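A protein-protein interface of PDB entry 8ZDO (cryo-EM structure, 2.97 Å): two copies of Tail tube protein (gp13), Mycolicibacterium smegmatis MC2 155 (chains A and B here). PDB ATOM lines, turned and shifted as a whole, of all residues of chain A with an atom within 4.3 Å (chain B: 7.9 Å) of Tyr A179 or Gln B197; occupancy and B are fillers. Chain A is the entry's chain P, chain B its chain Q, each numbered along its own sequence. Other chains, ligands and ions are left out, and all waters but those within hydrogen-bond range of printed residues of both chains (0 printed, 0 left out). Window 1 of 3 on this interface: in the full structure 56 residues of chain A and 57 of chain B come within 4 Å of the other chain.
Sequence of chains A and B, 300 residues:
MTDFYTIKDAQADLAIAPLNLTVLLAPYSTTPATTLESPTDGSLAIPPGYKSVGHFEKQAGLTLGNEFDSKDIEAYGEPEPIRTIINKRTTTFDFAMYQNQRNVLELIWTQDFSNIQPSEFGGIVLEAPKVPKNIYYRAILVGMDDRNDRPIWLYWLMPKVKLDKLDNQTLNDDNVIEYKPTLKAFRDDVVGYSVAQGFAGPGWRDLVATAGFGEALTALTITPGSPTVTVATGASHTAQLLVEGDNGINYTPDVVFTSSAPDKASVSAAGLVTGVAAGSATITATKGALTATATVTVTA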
ATOM      1  N   PHE A  95      10.622   7.228  19.159  1.00  0.00           N
ATOM      2  CA  PHE A  95      11.476   7.651  20.260  1.00  0.00           C
ATOM      3  C   PHE A  95      11.848   9.104  20.007  1.00  0.00           C
ATOM      4  O   PHE A  95      11.675   9.614  18.899  1.00  0.00           O
ATOM      5  CB  PHE A  95      12.725   6.770  20.380  1.00  0.00           C
ATOM      6  CG  PHE A  95      13.531   6.669  19.111  1.00  0.00           C
ATOM      7  CD1 PHE A  95      13.057   5.957  18.023  1.00  0.00           C
ATOM      8  CD2 PHE A  95      14.769   7.271  19.013  1.00  0.00           C
ATOM      9  CE1 PHE A  95      13.791   5.864  16.865  1.00  0.00           C
ATOM     10  CE2 PHE A  95      15.507   7.170  17.856  1.00  0.00           C
ATOM     11  CZ  PHE A  95      15.016   6.472  16.781  1.00  0.00           C
ATOM     12  N   ALA A  96      12.362   9.768  21.039  1.00  0.00           N
ATOM     13  CA  ALA A  96      12.636  11.205  20.987  1.00  0.00           C
ATOM     14  C   ALA A  96      14.124  11.456  21.202  1.00  0.00           C
ATOM     15  O   ALA A  96      14.586  11.540  22.342  1.00  0.00           O
ATOM     16  CB  ALA A  96      11.799  11.952  22.020  1.00  0.00           C
ATOM     17  N   MET A  97      14.860  11.616  20.106  1.00  0.00           N
ATOM     18  CA  MET A  97      16.296  11.849  20.172  1.00  0.00           C
ATOM     19  C   MET A  97      16.606  13.268  20.630  1.00  0.00           C
ATOM     20  O   MET A  97      15.895  14.217  20.292  1.00  0.00           O
ATOM     21  CB  MET A  97      16.926  11.602  18.806  1.00  0.00           C
ATOM     22  CG  MET A  97      16.431  10.349  18.139  1.00  0.00           C
ATOM     23  SD  MET A  97      16.983  10.156  16.439  1.00  0.00           S
ATOM     24  CE  MET A  97      15.926  11.335  15.613  1.00  0.00           C
ATOM     25  N   GLN A  99      20.238  14.510  20.631  1.00  0.00           N
ATOM     26  CA  GLN A  99      21.444  15.047  20.027  1.00  0.00           C
ATOM     27  C   GLN A  99      21.168  15.598  18.631  1.00  0.00           C
ATOM     28  O   GLN A  99      20.203  15.229  17.961  1.00  0.00           O
ATOM     29  CB  GLN A  99      22.528  13.975  19.971  1.00  0.00           C
ATOM     30  CG  GLN A  99      22.877  13.407  21.328  1.00  0.00           C
ATOM     31  CD  GLN A  99      24.003  12.406  21.264  1.00  0.00           C
ATOM     32  OE1 GLN A  99      24.389  11.825  22.274  1.00  0.00           O
ATOM     33  NE2 GLN A  99      24.540  12.197  20.069  1.00  0.00           N
ATOM     34  N   ASN A 100      22.048  16.497  18.200  1.00  0.00           N
ATOM     35  CA  ASN A 100      21.916  17.221  16.941  1.00  0.00           C
ATOM     36  C   ASN A 100      23.001  16.810  15.956  1.00  0.00           C
ATOM     37  O   ASN A 100      23.595  17.645  15.274  1.00  0.00           O
ATOM     38  CB  ASN A 100      21.956  18.727  17.180  1.00  0.00           C
ATOM     39  CG  ASN A 100      20.713  19.237  17.868  1.00  0.00           C
ATOM     40  OD1 ASN A 100      19.810  19.766  17.224  1.00  0.00           O
ATOM     41  ND2 ASN A 100      20.657  19.079  19.181  1.00  0.00           N
ATOM     42  N   VAL A 104      21.140  11.877  12.820  1.00  0.00           N
ATOM     43  CA  VAL A 104      19.836  12.287  13.338  1.00  0.00           C
ATOM     44  C   VAL A 104      19.217  13.342  12.431  1.00  0.00           C
ATOM     45  O   VAL A 104      18.042  13.255  12.054  1.00  0.00           O
ATOM     46  CB  VAL A 104      19.973  12.798  14.782  1.00  0.00           C
ATOM     47  CG1 VAL A 104      18.738  13.575  15.191  1.00  0.00           C
ATOM     48  CG2 VAL A 104      20.220  11.647  15.732  1.00  0.00           C
ATOM     49  N   LEU A 105      20.006  14.350  12.054  1.00  0.00           N
ATOM     50  CA  LEU A 105      19.477  15.422  11.216  1.00  0.00           C
ATOM     51  C   LEU A 105      19.133  14.920   9.818  1.00  0.00           C
ATOM     52  O   LEU A 105      18.135  15.350   9.228  1.00  0.00           O
ATOM     53  CB  LEU A 105      20.474  16.575  11.156  1.00  0.00           C
ATOM     54  CG  LEU A 105      20.630  17.317  12.486  1.00  0.00           C
ATOM     55  CD1 LEU A 105      21.814  18.263  12.458  1.00  0.00           C
ATOM     56  CD2 LEU A 105      19.355  18.063  12.830  1.00  0.00           C
ATOM     57  N   ILE A 108      15.867  13.150  10.095  1.00  0.00           N
ATOM     58  CA  ILE A 108      14.770  14.091  10.298  1.00  0.00           C
ATOM     59  C   ILE A 108      14.408  14.796   8.997  1.00  0.00           C
ATOM     60  O   ILE A 108      13.226  14.952   8.671  1.00  0.00           O
ATOM     61  CB  ILE A 108      15.134  15.094  11.407  1.00  0.00           C
ATOM     62  CG1 ILE A 108      15.156  14.392  12.764  1.00  0.00           C
ATOM     63  CG2 ILE A 108      14.166  16.260  11.421  1.00  0.00           C
ATOM     64  CD1 ILE A 108      13.970  13.498  13.003  1.00  0.00           C
ATOM     65  N   TRP A 109      15.405  15.228   8.232  1.00  0.00           N
ATOM     66  CA  TRP A 109      15.158  16.048   7.055  1.00  0.00           C
ATOM     67  C   TRP A 109      15.050  15.249   5.764  1.00  0.00           C
ATOM     68  O   TRP A 109      14.814  15.850   4.711  1.00  0.00           O
ATOM     69  CB  TRP A 109      16.258  17.102   6.915  1.00  0.00           C
ATOM     70  CG  TRP A 109      16.181  18.162   7.961  1.00  0.00           C
ATOM     71  CD1 TRP A 109      17.081  18.399   8.954  1.00  0.00           C
ATOM     72  CD2 TRP A 109      15.137  19.126   8.128  1.00  0.00           C
ATOM     73  NE1 TRP A 109      16.667  19.452   9.728  1.00  0.00           N
ATOM     74  CE2 TRP A 109      15.475  19.916   9.241  1.00  0.00           C
ATOM     75  CE3 TRP A 109      13.951  19.397   7.443  1.00  0.00           C
ATOM     76  CZ2 TRP A 109      14.670  20.961   9.684  1.00  0.00           C
ATOM     77  CZ3 TRP A 109      13.154  20.430   7.885  1.00  0.00           C
ATOM     78  CH2 TRP A 109      13.516  21.201   8.993  1.00  0.00           C
ATOM     79  N   VAL A 125      24.362  25.105   7.393  1.00  0.00           N
ATOM     80  CA  VAL A 125      22.971  25.358   7.043  1.00  0.00           C
ATOM     81  C   VAL A 125      22.443  24.122   6.331  1.00  0.00           C
ATOM     82  O   VAL A 125      23.028  23.678   5.337  1.00  0.00           O
ATOM     83  CB  VAL A 125      22.813  26.606   6.160  1.00  0.00           C
ATOM     84  CG1 VAL A 125      21.389  26.719   5.652  1.00  0.00           C
ATOM     85  CG2 VAL A 125      23.199  27.851   6.933  1.00  0.00           C
ATOM     86  N   LEU A 126      21.345  23.571   6.835  1.00  0.00           N
ATOM     87  CA  LEU A 126      20.763  22.338   6.316  1.00  0.00           C
ATOM     88  C   LEU A 126      19.413  22.666   5.691  1.00  0.00           C
ATOM     89  O   LEU A 126      18.429  22.888   6.400  1.00  0.00           O
ATOM     90  CB  LEU A 126      20.619  21.302   7.424  1.00  0.00           C
ATOM     91  CG  LEU A 126      21.868  21.077   8.269  1.00  0.00           C
ATOM     92  CD1 LEU A 126      21.589  20.043   9.332  1.00  0.00           C
ATOM     93  CD2 LEU A 126      23.029  20.653   7.395  1.00  0.00           C
ATOM     94  N   GLN A 169       7.409  19.588  17.220  1.00  0.00           N
ATOM     95  CA  GLN A 169       8.385  19.866  18.262  1.00  0.00           C
ATOM     96  C   GLN A 169       8.143  21.258  18.827  1.00  0.00           C
ATOM     97  O   GLN A 169       7.969  22.219  18.071  1.00  0.00           O
ATOM     98  CB  GLN A 169       9.811  19.739  17.726  1.00  0.00           C
ATOM     99  CG  GLN A 169      10.051  20.439  16.411  1.00  0.00           C
ATOM    100  CD  GLN A 169      11.467  20.257  15.917  1.00  0.00           C
ATOM    101  OE1 GLN A 169      12.319  19.730  16.628  1.00  0.00           O
ATOM    102  NE2 GLN A 169      11.726  20.688  14.690  1.00  0.00           N
ATOM    103  N   ILE A 177      15.970  20.758  22.665  1.00  0.00           N
ATOM    104  CA  ILE A 177      15.232  20.444  21.448  1.00  0.00           C
ATOM    105  C   ILE A 177      15.370  18.956  21.164  1.00  0.00           C
ATOM    106  O   ILE A 177      16.483  18.429  21.072  1.00  0.00           O
ATOM    107  CB  ILE A 177      15.731  21.285  20.266  1.00  0.00           C
ATOM    108  CG1 ILE A 177      15.118  22.677  20.335  1.00  0.00           C
ATOM    109  CG2 ILE A 177      15.381  20.622  18.948  1.00  0.00           C
ATOM    110  CD1 ILE A 177      15.519  23.563  19.208  1.00  0.00           C
ATOM    111  N   GLU A 178      14.237  18.278  21.025  1.00  0.00           N
ATOM    112  CA  GLU A 178      14.207  16.854  20.735  1.00  0.00           C
ATOM    113  C   GLU A 178      13.466  16.619  19.429  1.00  0.00           C
ATOM    114  O   GLU A 178      12.516  17.334  19.101  1.00  0.00           O
ATOM    115  CB  GLU A 178      13.542  16.064  21.869  1.00  0.00           C
ATOM    116  CG  GLU A 178      12.073  16.373  22.073  1.00  0.00           C
ATOM    117  CD  GLU A 178      11.585  16.005  23.459  1.00  0.00           C
ATOM    118  OE1 GLU A 178      12.358  16.171  24.425  1.00  0.00           O
ATOM    119  OE2 GLU A 178      10.427  15.553  23.584  1.00  0.00           O
ATOM    120  N   TYR A 179      13.922  15.622  18.683  1.00  0.00           N
ATOM    121  CA  TYR A 179      13.287  15.202  17.442  1.00  0.00           C
ATOM    122  C   TYR A 179      12.683  13.828  17.675  1.00  0.00           C
ATOM    123  O   TYR A 179      13.405  12.883  17.999  1.00  0.00           O
ATOM    124  CB  TYR A 179      14.292  15.159  16.293  1.00  0.00           C
ATOM    125  CG  TYR A 179      15.190  16.372  16.213  1.00  0.00           C
ATOM    126  CD1 TYR A 179      16.355  16.449  16.963  1.00  0.00           C
ATOM    127  CD2 TYR A 179      14.875  17.436  15.385  1.00  0.00           C
ATOM    128  CE1 TYR A 179      17.173  17.552  16.895  1.00  0.00           C
ATOM    129  CE2 TYR A 179      15.689  18.541  15.309  1.00  0.00           C
ATOM    130  CZ  TYR A 179      16.836  18.595  16.065  1.00  0.00           C
ATOM    131  OH  TYR A 179      17.653  19.698  15.992  1.00  0.00           O
ATOM    132  N   LYS A 180      11.366  13.714  17.524  1.00  0.00           N
ATOM    133  CA  LYS A 180      10.680  12.455  17.793  1.00  0.00           C
ATOM    134  C   LYS A 180      10.137  11.883  16.493  1.00  0.00           C
ATOM    135  O   LYS A 180       9.017  12.214  16.080  1.00  0.00           O
ATOM    136  CB  LYS A 180       9.557  12.645  18.815  1.00  0.00           C
ATOM    137  CG  LYS A 180       8.898  11.341  19.229  1.00  0.00           C
ATOM    138  CD  LYS A 180       7.886  11.541  20.338  1.00  0.00           C
ATOM    139  CE  LYS A 180       7.255  10.221  20.740  1.00  0.00           C
ATOM    140  NZ  LYS A 180       6.249  10.395  21.824  1.00  0.00           N
ATOM    141  N   PRO A 181      10.887  11.027  15.809  1.00  0.00           N
ATOM    142  CA  PRO A 181      10.385  10.397  14.591  1.00  0.00           C
ATOM    143  C   PRO A 181       9.745   9.042  14.861  1.00  0.00           C
ATOM    144  O   PRO A 181      10.020   8.373  15.858  1.00  0.00           O
ATOM    145  CB  PRO A 181      11.660  10.228  13.760  1.00  0.00           C
ATOM    146  CG  PRO A 181      12.716   9.995  14.772  1.00  0.00           C
ATOM    147  CD  PRO A 181      12.305  10.705  16.039  1.00  0.00           C
ATOM    148  N   LEU B  14      25.783  17.679  22.606  1.00  0.00           N
ATOM    149  CA  LEU B  14      25.026  17.825  21.373  1.00  0.00           C
ATOM    150  C   LEU B  14      23.547  18.084  21.620  1.00  0.00           C
ATOM    151  O   LEU B  14      22.786  18.191  20.653  1.00  0.00           O
ATOM    152  CB  LEU B  14      25.198  16.582  20.501  1.00  0.00           C
ATOM    153  CG  LEU B  14      26.480  16.520  19.675  1.00  0.00           C
ATOM    154  CD1 LEU B  14      26.412  15.378  18.684  1.00  0.00           C
ATOM    155  CD2 LEU B  14      26.712  17.834  18.959  1.00  0.00           C
ATOM    156  N   ALA B  15      23.123  18.165  22.877  1.00  0.00           N
ATOM    157  CA  ALA B  15      21.761  18.561  23.218  1.00  0.00           C
ATOM    158  C   ALA B  15      21.739  20.075  23.399  1.00  0.00           C
ATOM    159  O   ALA B  15      22.367  20.605  24.320  1.00  0.00           O
ATOM    160  CB  ALA B  15      21.287  17.844  24.477  1.00  0.00           C
ATOM    161  N   ILE B  16      21.015  20.767  22.527  1.00  0.00           N
ATOM    162  CA  ILE B  16      20.983  22.224  22.503  1.00  0.00           C
ATOM    163  C   ILE B  16      19.609  22.677  22.971  1.00  0.00           C
ATOM    164  O   ILE B  16      18.588  22.285  22.396  1.00  0.00           O
ATOM    165  CB  ILE B  16      21.300  22.769  21.103  1.00  0.00           C
ATOM    166  CG1 ILE B  16      22.617  22.182  20.597  1.00  0.00           C
ATOM    167  CG2 ILE B  16      21.375  24.281  21.130  1.00  0.00           C
ATOM    168  CD1 ILE B  16      22.748  22.186  19.099  1.00  0.00           C
ATOM    169  N   LEU B  64       6.870  24.012  16.201  1.00  0.00           N
ATOM    170  CA  LEU B  64       7.147  23.755  14.794  1.00  0.00           C
ATOM    171  C   LEU B  64       6.438  22.464  14.407  1.00  0.00           C
ATOM    172  O   LEU B  64       6.813  21.381  14.868  1.00  0.00           O
ATOM    173  CB  LEU B  64       8.648  23.642  14.541  1.00  0.00           C
ATOM    174  CG  LEU B  64       9.517  24.878  14.755  1.00  0.00           C
ATOM    175  CD1 LEU B  64      10.891  24.469  15.245  1.00  0.00           C
ATOM    176  CD2 LEU B  64       9.623  25.673  13.472  1.00  0.00           C
ATOM    177  N   ASN B  66       5.285  19.624  11.703  1.00  0.00           N
ATOM    178  CA  ASN B  66       5.623  18.932  10.468  1.00  0.00           C
ATOM    179  C   ASN B  66       4.511  17.948  10.147  1.00  0.00           C
ATOM    180  O   ASN B  66       4.167  17.104  10.980  1.00  0.00           O
ATOM    181  CB  ASN B  66       6.956  18.193  10.596  1.00  0.00           C
ATOM    182  CG  ASN B  66       8.134  19.133  10.722  1.00  0.00           C
ATOM    183  OD1 ASN B  66       8.410  19.926   9.823  1.00  0.00           O
ATOM    184  ND2 ASN B  66       8.829  19.060  11.850  1.00  0.00           N
ATOM    185  N   LEU B 141      13.741  32.306  12.723  1.00  0.00           N
ATOM    186  CA  LEU B 141      13.509  31.887  14.102  1.00  0.00           C
ATOM    187  C   LEU B 141      14.854  31.475  14.678  1.00  0.00           C
ATOM    188  O   LEU B 141      15.315  30.359  14.442  1.00  0.00           O
ATOM    189  CB  LEU B 141      12.509  30.741  14.166  1.00  0.00           C
ATOM    190  CG  LEU B 141      11.178  30.971  13.460  1.00  0.00           C
ATOM    191  CD1 LEU B 141      11.169  30.312  12.094  1.00  0.00           C
ATOM    192  CD2 LEU B 141      10.066  30.428  14.317  1.00  0.00           C
ATOM    193  N   LEU B 154      21.090  28.473  17.095  1.00  0.00           N
ATOM    194  CA  LEU B 154      20.430  27.541  16.196  1.00  0.00           C
ATOM    195  C   LEU B 154      19.185  28.211  15.639  1.00  0.00           C
ATOM    196  O   LEU B 154      18.396  28.788  16.391  1.00  0.00           O
ATOM    197  CB  LEU B 154      20.090  26.230  16.907  1.00  0.00           C
ATOM    198  CG  LEU B 154      18.975  26.132  17.947  1.00  0.00           C
ATOM    199  CD1 LEU B 154      18.654  24.675  18.157  1.00  0.00           C
ATOM    200  CD2 LEU B 154      19.373  26.776  19.262  1.00  0.00           C
ATOM    201  N   TYR B 155      19.023  28.162  14.321  1.00  0.00           N
ATOM    202  CA  TYR B 155      18.017  28.985  13.677  1.00  0.00           C
ATOM    203  C   TYR B 155      17.315  28.224  12.565  1.00  0.00           C
ATOM    204  O   TYR B 155      17.840  27.264  11.997  1.00  0.00           O
ATOM    205  CB  TYR B 155      18.625  30.278  13.123  1.00  0.00           C
ATOM    206  CG  TYR B 155      19.833  30.079  12.241  1.00  0.00           C
ATOM    207  CD1 TYR B 155      21.102  29.972  12.787  1.00  0.00           C
ATOM    208  CD2 TYR B 155      19.706  30.018  10.861  1.00  0.00           C
ATOM    209  CE1 TYR B 155      22.208  29.798  11.986  1.00  0.00           C
ATOM    210  CE2 TYR B 155      20.808  29.844  10.052  1.00  0.00           C
ATOM    211  CZ  TYR B 155      22.057  29.735  10.620  1.00  0.00           C
ATOM    212  OH  TYR B 155      23.161  29.561   9.823  1.00  0.00           O
ATOM    213  N   TRP B 156      16.100  28.675  12.278  1.00  0.00           N
ATOM    214  CA  TRP B 156      15.294  28.211  11.161  1.00  0.00           C
ATOM    215  C   TRP B 156      15.065  29.383  10.221  1.00  0.00           C
ATOM    216  O   TRP B 156      14.640  30.458  10.655  1.00  0.00           O
ATOM    217  CB  TRP B 156      13.953  27.647  11.633  1.00  0.00           C
ATOM    218  CG  TRP B 156      14.071  26.385  12.416  1.00  0.00           C
ATOM    219  CD1 TRP B 156      13.808  25.125  11.980  1.00  0.00           C
ATOM    220  CD2 TRP B 156      14.481  26.261  13.780  1.00  0.00           C
ATOM    221  NE1 TRP B 156      14.033  24.220  12.986  1.00  0.00           N
ATOM    222  CE2 TRP B 156      14.448  24.895  14.102  1.00  0.00           C
ATOM    223  CE3 TRP B 156      14.878  27.175  14.759  1.00  0.00           C
ATOM    224  CZ2 TRP B 156      14.794  24.421  15.359  1.00  0.00           C
ATOM    225  CZ3 TRP B 156      15.224  26.702  16.002  1.00  0.00           C
ATOM    226  CH2 TRP B 156      15.179  25.340  16.292  1.00  0.00           C
ATOM    227  N   LEU B 157      15.356  29.174   8.946  1.00  0.00           N
ATOM    228  CA  LEU B 157      15.140  30.170   7.907  1.00  0.00           C
ATOM    229  C   LEU B 157      13.974  29.713   7.048  1.00  0.00           C
ATOM    230  O   LEU B 157      14.022  28.626   6.462  1.00  0.00           O
ATOM    231  CB  LEU B 157      16.392  30.357   7.053  1.00  0.00           C
ATOM    232  CG  LEU B 157      17.677  30.754   7.772  1.00  0.00           C
ATOM    233  CD1 LEU B 157      18.850  30.678   6.820  1.00  0.00           C
ATOM    234  CD2 LEU B 157      17.555  32.142   8.360  1.00  0.00           C
ATOM    235  N   MET B 158      12.927  30.532   6.984  1.00  0.00           N
ATOM    236  CA  MET B 158      11.762  30.252   6.148  1.00  0.00           C
ATOM    237  C   MET B 158      11.566  31.421   5.198  1.00  0.00           C
ATOM    238  O   MET B 158      10.969  32.442   5.578  1.00  0.00           O
ATOM    239  CB  MET B 158      10.519  30.026   7.005  1.00  0.00           C
ATOM    240  CG  MET B 158      10.700  28.946   8.054  1.00  0.00           C
ATOM    241  SD  MET B 158       9.184  28.545   8.932  1.00  0.00           S
ATOM    242  CE  MET B 158       9.812  27.445  10.194  1.00  0.00           C
ATOM    243  N   TYR B 193      14.173  26.495  -1.314  1.00  0.00           N
ATOM    244  CA  TYR B 193      13.746  25.694  -0.178  1.00  0.00           C
ATOM    245  C   TYR B 193      12.631  26.419   0.557  1.00  0.00           C
ATOM    246  O   TYR B 193      12.452  27.631   0.416  1.00  0.00           O
ATOM    247  CB  TYR B 193      14.912  25.377   0.769  1.00  0.00           C
ATOM    248  CG  TYR B 193      15.552  26.582   1.414  1.00  0.00           C
ATOM    249  CD1 TYR B 193      15.048  27.117   2.589  1.00  0.00           C
ATOM    250  CD2 TYR B 193      16.670  27.178   0.856  1.00  0.00           C
ATOM    251  CE1 TYR B 193      15.630  28.214   3.181  1.00  0.00           C
ATOM    252  CE2 TYR B 193      17.262  28.275   1.443  1.00  0.00           C
ATOM    253  CZ  TYR B 193      16.739  28.789   2.604  1.00  0.00           C
ATOM    254  OH  TYR B 193      17.324  29.884   3.196  1.00  0.00           O
ATOM    255  N   VAL B 195      12.042  25.543   4.172  1.00  0.00           N
ATOM    256  CA  VAL B 195      12.568  25.690   5.521  1.00  0.00           C
ATOM    257  C   VAL B 195      13.990  25.152   5.538  1.00  0.00           C
ATOM    258  O   VAL B 195      14.298  24.154   4.880  1.00  0.00           O
ATOM    259  CB  VAL B 195      11.677  24.971   6.560  1.00  0.00           C
ATOM    260  CG1 VAL B 195      11.594  23.486   6.266  1.00  0.00           C
ATOM    261  CG2 VAL B 195      12.191  25.208   7.968  1.00  0.00           C
ATOM    262  N   ALA B 196      14.867  25.835   6.265  1.00  0.00           N
ATOM    263  CA  ALA B 196      16.233  25.381   6.461  1.00  0.00           C
ATOM    264  C   ALA B 196      16.606  25.530   7.925  1.00  0.00           C
ATOM    265  O   ALA B 196      16.129  26.435   8.609  1.00  0.00           O
ATOM    266  CB  ALA B 196      17.219  26.163   5.594  1.00  0.00           C
ATOM    267  N   GLN B 197      17.462  24.636   8.402  1.00  0.00           N
ATOM    268  CA  GLN B 197      17.933  24.667   9.777  1.00  0.00           C
ATOM    269  C   GLN B 197      19.438  24.865   9.784  1.00  0.00           C
ATOM    270  O   GLN B 197      20.158  24.258   8.987  1.00  0.00           O
ATOM    271  CB  GLN B 197      17.561  23.382  10.518  1.00  0.00           C
ATOM    272  CG  GLN B 197      17.887  23.408  11.996  1.00  0.00           C
ATOM    273  CD  GLN B 197      17.525  22.117  12.690  1.00  0.00           C
ATOM    274  OE1 GLN B 197      16.917  21.230  12.094  1.00  0.00           O
ATOM    275  NE2 GLN B 197      17.898  22.002  13.956  1.00  0.00           N
ATOM    276  N   GLY B 198      19.914  25.726  10.681  1.00  0.00           N
ATOM    277  CA  GLY B 198      21.321  26.049  10.731  1.00  0.00           C
ATOM    278  C   GLY B 198      21.802  26.220  12.156  1.00  0.00           C
ATOM    279  O   GLY B 198      21.022  26.450  13.081  1.00  0.00           O
ATOM    280  N   PHE B 199      23.121  26.115  12.308  1.00  0.00           N
ATOM    281  CA  PHE B 199      23.797  26.258  13.586  1.00  0.00           C
ATOM    282  C   PHE B 199      24.990  27.186  13.411  1.00  0.00           C
ATOM    283  O   PHE B 199      25.590  27.244  12.338  1.00  0.00           O
ATOM    284  CB  PHE B 199      24.280  24.909  14.132  1.00  0.00           C
ATOM    285  CG  PHE B 199      23.200  23.872  14.255  1.00  0.00           C
ATOM    286  CD1 PHE B 199      22.797  23.135  13.155  1.00  0.00           C
ATOM    287  CD2 PHE B 199      22.604  23.620  15.474  1.00  0.00           C
ATOM    288  CE1 PHE B 199      21.808  22.182  13.269  1.00  0.00           C
ATOM    289  CE2 PHE B 199      21.618  22.666  15.593  1.00  0.00           C
ATOM    290  CZ  PHE B 199      21.220  21.949  14.490  1.00  0.00           C
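Along chain A the printed residues that touch a printed residue of chain B span positions 99 to 179.
Printed residues of chain B that touch a printed residue of chain A: Leu B14, Ile B16, Leu B64, Leu B154, Tyr B155, Trp B156, Val B195, Ala B196, Gln B197 and Phe B199.
Hydrophobic or aromatic side chains of chain B within 4 Å of the printed part of chain A: Leu B14, Ile B16, Leu B64, Leu B154, Tyr B155, Trp B156, Val B195, Ala B196 and Phe B199.
Among the printed residues, pairs that only touch across the chains: Gln A99 with Leu B14, Asn A100 with Ile B16, Asn A100 with Phe B199, Trp A109 with Val B195, Val A125 with Tyr B155, Val A125 with Gln B197, Leu A126 with Ala B196, Ile A177 with Leu B154 and Ile A177 with Trp B156.
Of chain B, only Gln B197 comes within 4 Å of Tyr A179.
Of the printed residues of chain A, Ile B16 touches Asn A100 (3.7 Å) and Ile A177 (3.0 Å).
Of chain A, only Trp A109 (3.0 Å), Val A125 (3.5 Å), Leu A126 (2.6 Å) and Tyr A179 (3.1 Å) come within 4 Å of Gln B197.
Printed residues of chain A within 4 Å of Phe B199: Asn A100 (3.8 Å).
The nearest residue of chain B that does not touch Tyr A179 is Phe B199 (4.5 Å).
The nearest printed residue of chain A that does not touch Leu B64 is Ile A177 (6.2 Å).
The backbone carbonyl oxygen (O) of Gln A169 lies within hydrogen-bond range of the backbone NH (N) of Leu B64 (2.8 Å).
The side-chain amide oxygen (OE1) of Gln B197 sits at hydrogen-bond distance from the indole nitrogen (NE1) of Trp A109, 3.0 Å away.
O of Leu B14 lies within hydrogen-bond range of ND2 of Asn A100 (2.7 Å).
The side-chain amide nitrogen (NE2) of Gln B197 is in hydrogen-bond range of the side-chain hydroxyl (OH) of Tyr A179 (3.1 Å).
The backbone carbonyl oxygen (O) of Gln B197 sits at hydrogen-bond distance from the backbone NH (N) of Leu A126, at 2.6 Å.
N of Ile A177 lies within hydrogen-bond range of O of Ile B16, 3.0 Å away.
N of Leu B157 lies within hydrogen-bond range of O of Ala B196 (2.9 Å).
N of Trp B156 lies within hydrogen-bond range of O of Leu B141 (2.9 Å).
The backbone carbonyl oxygen (O) of Glu A178 sits close to the side-chain amide oxygen (OE1) of Gln A169, 3.4 Å away.
The backbone NH (N) of Gly B198 sits at hydrogen-bond distance from the backbone carbonyl oxygen (O) of Tyr B155 (2.9 Å).
The side-chain amide oxygen of Asn A100 sits at hydrogen-bond distance from the side-chain hydroxyl of Tyr A179 (2.5 Å).
N of Met A97 sits at hydrogen-bond distance from O of Tyr A179 (2.9 Å).
No position is printed for both chains.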
